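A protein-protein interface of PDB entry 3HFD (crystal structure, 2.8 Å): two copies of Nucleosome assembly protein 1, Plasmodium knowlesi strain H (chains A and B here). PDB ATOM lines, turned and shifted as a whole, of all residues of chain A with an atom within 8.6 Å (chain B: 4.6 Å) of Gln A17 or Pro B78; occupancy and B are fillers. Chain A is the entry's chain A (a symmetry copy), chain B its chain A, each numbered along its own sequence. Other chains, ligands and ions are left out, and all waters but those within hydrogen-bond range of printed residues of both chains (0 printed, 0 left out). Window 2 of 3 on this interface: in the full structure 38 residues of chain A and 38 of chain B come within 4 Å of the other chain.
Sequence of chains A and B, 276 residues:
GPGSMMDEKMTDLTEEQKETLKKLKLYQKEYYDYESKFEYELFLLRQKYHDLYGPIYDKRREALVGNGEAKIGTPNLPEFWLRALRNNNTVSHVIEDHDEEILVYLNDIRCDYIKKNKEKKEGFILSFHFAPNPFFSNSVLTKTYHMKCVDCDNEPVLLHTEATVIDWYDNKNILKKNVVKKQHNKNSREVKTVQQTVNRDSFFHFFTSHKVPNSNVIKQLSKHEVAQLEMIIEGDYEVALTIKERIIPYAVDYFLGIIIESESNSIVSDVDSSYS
The backbone carbonyl oxygen of Asn B76 is in hydrogen-bond range of the side-chain hydroxyl of Thr A20, at 3.4 Å.
The side-chain hydroxyl of Thr B74 sits at hydrogen-bond distance from the backbone carbonyl oxygen of Leu B77 (3.0 Å). The side-chain amide oxygen (OE1) of Gln A17 lies within hydrogen-bond range of the backbone NH (N) of Thr A14 (3.0 Å). The backbone carbonyl oxygen (O) of Glu A16 is in hydrogen-bond range of the side-chain hydroxyl (OG1) of Thr A20 (3.3 Å).
Among the printed residues, merely in contact across the chains: Gln A17 with Pro B78, Leu A21 with Leu B77, Gln A17 with Leu B77, Leu A24 with Leu B77, Gln A17 with Asn B76, Leu A24 with Phe B80 and Thr A20 with Leu B77.
Glu A16 touches none of the printed residues of chain B. Of chain B, only Asn B76 (3.5 Å), Leu B77 (3.5 Å) and Pro B78 (3.3 Å) come within 4 Å of Gln A17. Lys A18 touches none of the printed residues of chain B. Of the printed residues of chain B, Thr A20 touches Asn B76 and Leu B77. Of the printed residues of chain B, Leu A21 touches Leu B77 (3.4 Å). Of the printed residues of chain A, Asn B76 touches Gln A17 and Thr A20. Printed residues of chain A within 4 Å of Pro B78: Gln A17. Of the printed residues of chain A, Phe B80 touches Leu A24 (3.6 Å). The nearest residue of chain A that does not touch Pro B78 is Leu A13 (6.4 Å). The nearest printed residue of chain A that does not touch Asn B76 is Glu A16 (4.6 Å).
Printed residues of chain B that touch a printed residue of chain A: Asn B76, Leu B77, Pro B78 and Phe B80. Hydrophobic or aromatic side chains of chain B within 4 Å of the printed part of chain A: Leu B77, Pro B78 and Phe B80. Hydrophobic or aromatic side chains of chain A within 4 Å of the printed part of chain B: Leu A21 and Leu A24.
No position is printed for both chains. Of the 8 pairs that touch across the chains among the printed residues, none has its exchanged pair printed and touching as well.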
ATOM      1  N   THR A  11     -17.508 -15.647 -14.280  1.00  0.00           N
ATOM      2  CA  THR A  11     -17.560 -14.527 -15.270  1.00  0.00           C
ATOM      3  C   THR A  11     -17.223 -13.171 -14.618  1.00  0.00           C
ATOM      4  O   THR A  11     -16.409 -12.402 -15.153  1.00  0.00           O
ATOM      5  CB  THR A  11     -18.955 -14.449 -15.966  1.00  0.00           C
ATOM      6  OG1 THR A  11     -19.983 -14.229 -14.989  1.00  0.00           O
ATOM      7  CG2 THR A  11     -19.261 -15.747 -16.744  1.00  0.00           C
ATOM      8  N   ASP A  12     -17.824 -12.902 -13.454  1.00  0.00           N
ATOM      9  CA  ASP A  12     -17.774 -11.570 -12.813  1.00  0.00           C
ATOM     10  C   ASP A  12     -17.085 -11.559 -11.423  1.00  0.00           C
ATOM     11  O   ASP A  12     -17.649 -11.065 -10.444  1.00  0.00           O
ATOM     12  CB  ASP A  12     -19.207 -11.021 -12.700  1.00  0.00           C
ATOM     13  CG  ASP A  12     -20.013 -11.192 -13.988  1.00  0.00           C
ATOM     14  OD1 ASP A  12     -19.588 -10.660 -15.041  1.00  0.00           O
ATOM     15  OD2 ASP A  12     -21.074 -11.855 -13.946  1.00  0.00           O
ATOM     16  N   LEU A  13     -15.860 -12.088 -11.354  1.00  0.00           N
ATOM     17  CA  LEU A  13     -15.134 -12.270 -10.082  1.00  0.00           C
ATOM     18  C   LEU A  13     -13.787 -11.543 -10.079  1.00  0.00           C
ATOM     19  O   LEU A  13     -13.237 -11.212 -11.135  1.00  0.00           O
ATOM     20  CB  LEU A  13     -14.860 -13.764  -9.815  1.00  0.00           C
ATOM     21  CG  LEU A  13     -15.885 -14.865 -10.149  1.00  0.00           C
ATOM     22  CD1 LEU A  13     -15.177 -16.191 -10.460  1.00  0.00           C
ATOM     23  CD2 LEU A  13     -16.912 -15.047  -9.028  1.00  0.00           C
ATOM     24  N   THR A  14     -13.230 -11.333  -8.890  1.00  0.00           N
ATOM     25  CA  THR A  14     -11.868 -10.823  -8.800  1.00  0.00           C
ATOM     26  C   THR A  14     -10.877 -11.972  -9.061  1.00  0.00           C
ATOM     27  O   THR A  14     -11.263 -13.140  -9.158  1.00  0.00           O
ATOM     28  CB  THR A  14     -11.583 -10.099  -7.445  1.00  0.00           C
ATOM     29  OG1 THR A  14     -11.435 -11.051  -6.383  1.00  0.00           O
ATOM     30  CG2 THR A  14     -12.696  -9.115  -7.107  1.00  0.00           C
ATOM     31  N   GLU A  15      -9.599 -11.635  -9.185  1.00  0.00           N
ATOM     32  CA  GLU A  15      -8.592 -12.636  -9.523  1.00  0.00           C
ATOM     33  C   GLU A  15      -8.322 -13.546  -8.310  1.00  0.00           C
ATOM     34  O   GLU A  15      -8.042 -14.730  -8.470  1.00  0.00           O
ATOM     35  CB  GLU A  15      -7.289 -11.989 -10.041  1.00  0.00           C
ATOM     36  CG  GLU A  15      -7.423 -10.742 -10.985  1.00  0.00           C
ATOM     37  CD  GLU A  15      -8.223 -10.959 -12.270  1.00  0.00           C
ATOM     38  OE1 GLU A  15      -7.960 -11.948 -13.003  1.00  0.00           O
ATOM     39  OE2 GLU A  15      -9.096 -10.107 -12.564  1.00  0.00           O
ATOM     40  N   GLU A  16      -8.417 -12.991  -7.103  1.00  0.00           N
ATOM     41  CA  GLU A  16      -8.301 -13.778  -5.872  1.00  0.00           C
ATOM     42  C   GLU A  16      -9.379 -14.833  -5.793  1.00  0.00           C
ATOM     43  O   GLU A  16      -9.158 -15.938  -5.303  1.00  0.00           O
ATOM     44  CB  GLU A  16      -8.533 -12.896  -4.660  1.00  0.00           C
ATOM     45  CG  GLU A  16      -7.458 -11.924  -4.299  1.00  0.00           C
ATOM     46  CD  GLU A  16      -7.937 -10.992  -3.191  1.00  0.00           C
ATOM     47  OE1 GLU A  16      -8.904 -10.221  -3.446  1.00  0.00           O
ATOM     48  OE2 GLU A  16      -7.363 -11.048  -2.077  1.00  0.00           O
ATOM     49  N   GLN A  17     -10.571 -14.431  -6.217  1.00  0.00           N
ATOM     50  CA  GLN A  17     -11.754 -15.262  -6.166  1.00  0.00           C
ATOM     51  C   GLN A  17     -11.695 -16.304  -7.258  1.00  0.00           C
ATOM     52  O   GLN A  17     -12.318 -17.357  -7.152  1.00  0.00           O
ATOM     53  CB  GLN A  17     -12.995 -14.384  -6.325  1.00  0.00           C
ATOM     54  CG  GLN A  17     -13.197 -13.399  -5.150  1.00  0.00           C
ATOM     55  CD  GLN A  17     -14.306 -12.385  -5.393  1.00  0.00           C
ATOM     56  OE1 GLN A  17     -14.831 -12.264  -6.503  1.00  0.00           O
ATOM     57  NE2 GLN A  17     -14.665 -11.649  -4.351  1.00  0.00           N
ATOM     58  N   LYS A  18     -10.947 -15.999  -8.314  1.00  0.00           N
ATOM     59  CA  LYS A  18     -10.692 -16.953  -9.379  1.00  0.00           C
ATOM     60  C   LYS A  18      -9.740 -18.056  -8.935  1.00  0.00           C
ATOM     61  O   LYS A  18      -9.966 -19.220  -9.237  1.00  0.00           O
ATOM     62  CB  LYS A  18     -10.132 -16.242 -10.609  1.00  0.00           C
ATOM     63  CG  LYS A  18     -11.134 -15.367 -11.330  1.00  0.00           C
ATOM     64  CD  LYS A  18     -10.467 -14.716 -12.537  1.00  0.00           C
ATOM     65  CE  LYS A  18     -11.026 -13.329 -12.867  1.00  0.00           C
ATOM     66  NZ  LYS A  18     -12.193 -13.416 -13.781  1.00  0.00           N
ATOM     67  N   GLU A  19      -8.677 -17.705  -8.224  1.00  0.00           N
ATOM     68  CA  GLU A  19      -7.751 -18.720  -7.693  1.00  0.00           C
ATOM     69  C   GLU A  19      -8.464 -19.648  -6.701  1.00  0.00           C
ATOM     70  O   GLU A  19      -8.184 -20.846  -6.644  1.00  0.00           O
ATOM     71  CB  GLU A  19      -6.514 -18.072  -7.039  1.00  0.00           C
ATOM     72  CG  GLU A  19      -5.264 -18.027  -7.943  1.00  0.00           C
ATOM     73  CD  GLU A  19      -4.649 -19.417  -8.199  1.00  0.00           C
ATOM     74  OE1 GLU A  19      -3.688 -19.502  -8.996  1.00  0.00           O
ATOM     75  OE2 GLU A  19      -5.116 -20.424  -7.606  1.00  0.00           O
ATOM     76  N   THR A  20      -9.393 -19.082  -5.934  1.00  0.00           N
ATOM     77  CA  THR A  20     -10.250 -19.865  -5.051  1.00  0.00           C
ATOM     78  C   THR A  20     -11.128 -20.829  -5.824  1.00  0.00           C
ATOM     79  O   THR A  20     -11.501 -21.880  -5.303  1.00  0.00           O
ATOM     80  CB  THR A  20     -11.167 -18.973  -4.217  1.00  0.00           C
ATOM     81  OG1 THR A  20     -10.379 -18.262  -3.258  1.00  0.00           O
ATOM     82  CG2 THR A  20     -12.217 -19.808  -3.492  1.00  0.00           C
ATOM     83  N   LEU A  21     -11.463 -20.466  -7.055  1.00  0.00           N
ATOM     84  CA  LEU A  21     -12.251 -21.332  -7.920  1.00  0.00           C
ATOM     85  C   LEU A  21     -11.399 -22.443  -8.534  1.00  0.00           C
ATOM     86  O   LEU A  21     -11.815 -23.592  -8.558  1.00  0.00           O
ATOM     87  CB  LEU A  21     -12.937 -20.510  -9.008  1.00  0.00           C
ATOM     88  CG  LEU A  21     -14.387 -20.862  -9.305  1.00  0.00           C
ATOM     89  CD1 LEU A  21     -15.206 -21.047  -8.035  1.00  0.00           C
ATOM     90  CD2 LEU A  21     -14.961 -19.746 -10.151  1.00  0.00           C
ATOM     91  N   LYS A  22     -10.212 -22.113  -9.027  1.00  0.00           N
ATOM     92  CA  LYS A  22      -9.273 -23.160  -9.418  1.00  0.00           C
ATOM     93  C   LYS A  22      -9.247 -24.222  -8.335  1.00  0.00           C
ATOM     94  O   LYS A  22      -9.518 -25.391  -8.591  1.00  0.00           O
ATOM     95  CB  LYS A  22      -7.853 -22.626  -9.626  1.00  0.00           C
ATOM     96  CG  LYS A  22      -7.426 -22.635 -11.051  1.00  0.00           C
ATOM     97  CD  LYS A  22      -5.977 -22.224 -11.213  1.00  0.00           C
ATOM     98  CE  LYS A  22      -5.027 -23.401 -11.322  1.00  0.00           C
ATOM     99  NZ  LYS A  22      -3.650 -22.894 -11.584  1.00  0.00           N
ATOM    100  N   LYS A  23      -8.927 -23.808  -7.118  1.00  0.00           N
ATOM    101  CA  LYS A  23      -8.809 -24.750  -6.019  1.00  0.00           C
ATOM    102  C   LYS A  23     -10.092 -25.580  -5.886  1.00  0.00           C
ATOM    103  O   LYS A  23     -10.039 -26.803  -5.786  1.00  0.00           O
ATOM    104  CB  LYS A  23      -8.465 -24.013  -4.720  1.00  0.00           C
ATOM    105  CG  LYS A  23      -6.967 -23.699  -4.578  1.00  0.00           C
ATOM    106  CD  LYS A  23      -6.690 -22.482  -3.684  1.00  0.00           C
ATOM    107  CE  LYS A  23      -7.046 -22.744  -2.216  1.00  0.00           C
ATOM    108  NZ  LYS A  23      -7.128 -21.488  -1.408  1.00  0.00           N
ATOM    109  N   LEU A  24     -11.240 -24.911  -5.931  1.00  0.00           N
ATOM    110  CA  LEU A  24     -12.528 -25.595  -5.821  1.00  0.00           C
ATOM    111  C   LEU A  24     -12.759 -26.553  -6.979  1.00  0.00           C
ATOM    112  O   LEU A  24     -13.186 -27.686  -6.764  1.00  0.00           O
ATOM    113  CB  LEU A  24     -13.686 -24.593  -5.717  1.00  0.00           C
ATOM    114  CG  LEU A  24     -14.098 -24.216  -4.289  1.00  0.00           C
ATOM    115  CD1 LEU A  24     -12.883 -24.027  -3.410  1.00  0.00           C
ATOM    116  CD2 LEU A  24     -14.981 -22.961  -4.266  1.00  0.00           C
ATOM    117  N   GLY B  73     -20.051 -14.471   4.958  1.00  0.00           N
ATOM    118  CA  GLY B  73     -19.923 -15.873   4.561  1.00  0.00           C
ATOM    119  C   GLY B  73     -18.955 -16.138   3.414  1.00  0.00           C
ATOM    120  O   GLY B  73     -18.913 -15.378   2.447  1.00  0.00           O
ATOM    121  N   THR B  74     -18.187 -17.228   3.530  1.00  0.00           N
ATOM    122  CA  THR B  74     -17.227 -17.665   2.509  1.00  0.00           C
ATOM    123  C   THR B  74     -16.478 -16.514   1.820  1.00  0.00           C
ATOM    124  O   THR B  74     -16.504 -16.405   0.588  1.00  0.00           O
ATOM    125  CB  THR B  74     -17.931 -18.501   1.446  1.00  0.00           C
ATOM    126  OG1 THR B  74     -18.982 -17.726   0.858  1.00  0.00           O
ATOM    127  CG2 THR B  74     -18.504 -19.778   2.062  1.00  0.00           C
ATOM    128  N   PRO B  75     -15.780 -15.671   2.609  1.00  0.00           N
ATOM    129  CA  PRO B  75     -15.187 -14.410   2.114  1.00  0.00           C
ATOM    130  C   PRO B  75     -14.271 -14.520   0.883  1.00  0.00           C
ATOM    131  O   PRO B  75     -14.154 -13.555   0.135  1.00  0.00           O
ATOM    132  CB  PRO B  75     -14.406 -13.872   3.332  1.00  0.00           C
ATOM    133  CG  PRO B  75     -14.265 -15.037   4.265  1.00  0.00           C
ATOM    134  CD  PRO B  75     -15.466 -15.898   4.031  1.00  0.00           C
ATOM    135  N   ASN B  76     -13.635 -15.668   0.675  1.00  0.00           N
ATOM    136  CA  ASN B  76     -12.797 -15.867  -0.509  1.00  0.00           C
ATOM    137  C   ASN B  76     -13.595 -16.138  -1.796  1.00  0.00           C
ATOM    138  O   ASN B  76     -13.040 -16.130  -2.889  1.00  0.00           O
ATOM    139  CB  ASN B  76     -11.797 -16.993  -0.258  1.00  0.00           C
ATOM    140  CG  ASN B  76     -10.899 -16.712   0.927  1.00  0.00           C
ATOM    141  OD1 ASN B  76     -10.741 -15.566   1.328  1.00  0.00           O
ATOM    142  ND2 ASN B  76     -10.318 -17.760   1.501  1.00  0.00           N
ATOM    143  N   LEU B  77     -14.893 -16.364  -1.661  1.00  0.00           N
ATOM    144  CA  LEU B  77     -15.777 -16.524  -2.808  1.00  0.00           C
ATOM    145  C   LEU B  77     -17.181 -16.175  -2.309  1.00  0.00           C
ATOM    146  O   LEU B  77     -17.963 -17.046  -1.922  1.00  0.00           O
ATOM    147  CB  LEU B  77     -15.692 -17.954  -3.353  1.00  0.00           C
ATOM    148  CG  LEU B  77     -16.260 -18.241  -4.740  1.00  0.00           C
ATOM    149  CD1 LEU B  77     -15.521 -17.410  -5.771  1.00  0.00           C
ATOM    150  CD2 LEU B  77     -16.154 -19.756  -5.051  1.00  0.00           C
ATOM    151  N   PRO B  78     -17.480 -14.870  -2.260  1.00  0.00           N
ATOM    152  CA  PRO B  78     -18.715 -14.405  -1.638  1.00  0.00           C
ATOM    153  C   PRO B  78     -19.972 -15.061  -2.203  1.00  0.00           C
ATOM    154  O   PRO B  78     -20.059 -15.292  -3.409  1.00  0.00           O
ATOM    155  CB  PRO B  78     -18.702 -12.900  -1.940  1.00  0.00           C
ATOM    156  CG  PRO B  78     -17.262 -12.556  -2.065  1.00  0.00           C
ATOM    157  CD  PRO B  78     -16.646 -13.742  -2.729  1.00  0.00           C
ATOM    158  N   GLU B  79     -20.918 -15.352  -1.316  1.00  0.00           N
ATOM    159  CA  GLU B  79     -22.237 -15.884  -1.678  1.00  0.00           C
ATOM    160  C   GLU B  79     -22.189 -17.260  -2.364  1.00  0.00           C
ATOM    161  O   GLU B  79     -23.067 -17.595  -3.164  1.00  0.00           O
ATOM    162  CB  GLU B  79     -23.005 -14.869  -2.538  1.00  0.00           C
ATOM    163  CG  GLU B  79     -22.865 -13.428  -2.047  1.00  0.00           C
ATOM    164  CD  GLU B  79     -23.918 -12.471  -2.603  1.00  0.00           C
ATOM    165  OE1 GLU B  79     -24.694 -12.857  -3.508  1.00  0.00           O
ATOM    166  OE2 GLU B  79     -23.961 -11.314  -2.122  1.00  0.00           O
ATOM    167  N   PHE B  80     -21.179 -18.063  -2.018  1.00  0.00           N
ATOM    168  CA  PHE B  80     -20.944 -19.372  -2.661  1.00  0.00           C
ATOM    169  C   PHE B  80     -22.065 -20.372  -2.373  1.00  0.00           C
ATOM    170  O   PHE B  80     -22.630 -20.986  -3.277  1.00  0.00           O
ATOM    171  CB  PHE B  80     -19.592 -19.964  -2.203  1.00  0.00           C
ATOM    172  CG  PHE B  80     -19.332 -21.374  -2.701  1.00  0.00           C
ATOM    173  CD1 PHE B  80     -18.821 -21.594  -3.961  1.00  0.00           C
ATOM    174  CD2 PHE B  80     -19.596 -22.465  -1.907  1.00  0.00           C
ATOM    175  CE1 PHE B  80     -18.585 -22.861  -4.406  1.00  0.00           C
ATOM    176  CE2 PHE B  80     -19.352 -23.747  -2.356  1.00  0.00           C
ATOM    177  CZ  PHE B  80     -18.848 -23.942  -3.593  1.00  0.00           C
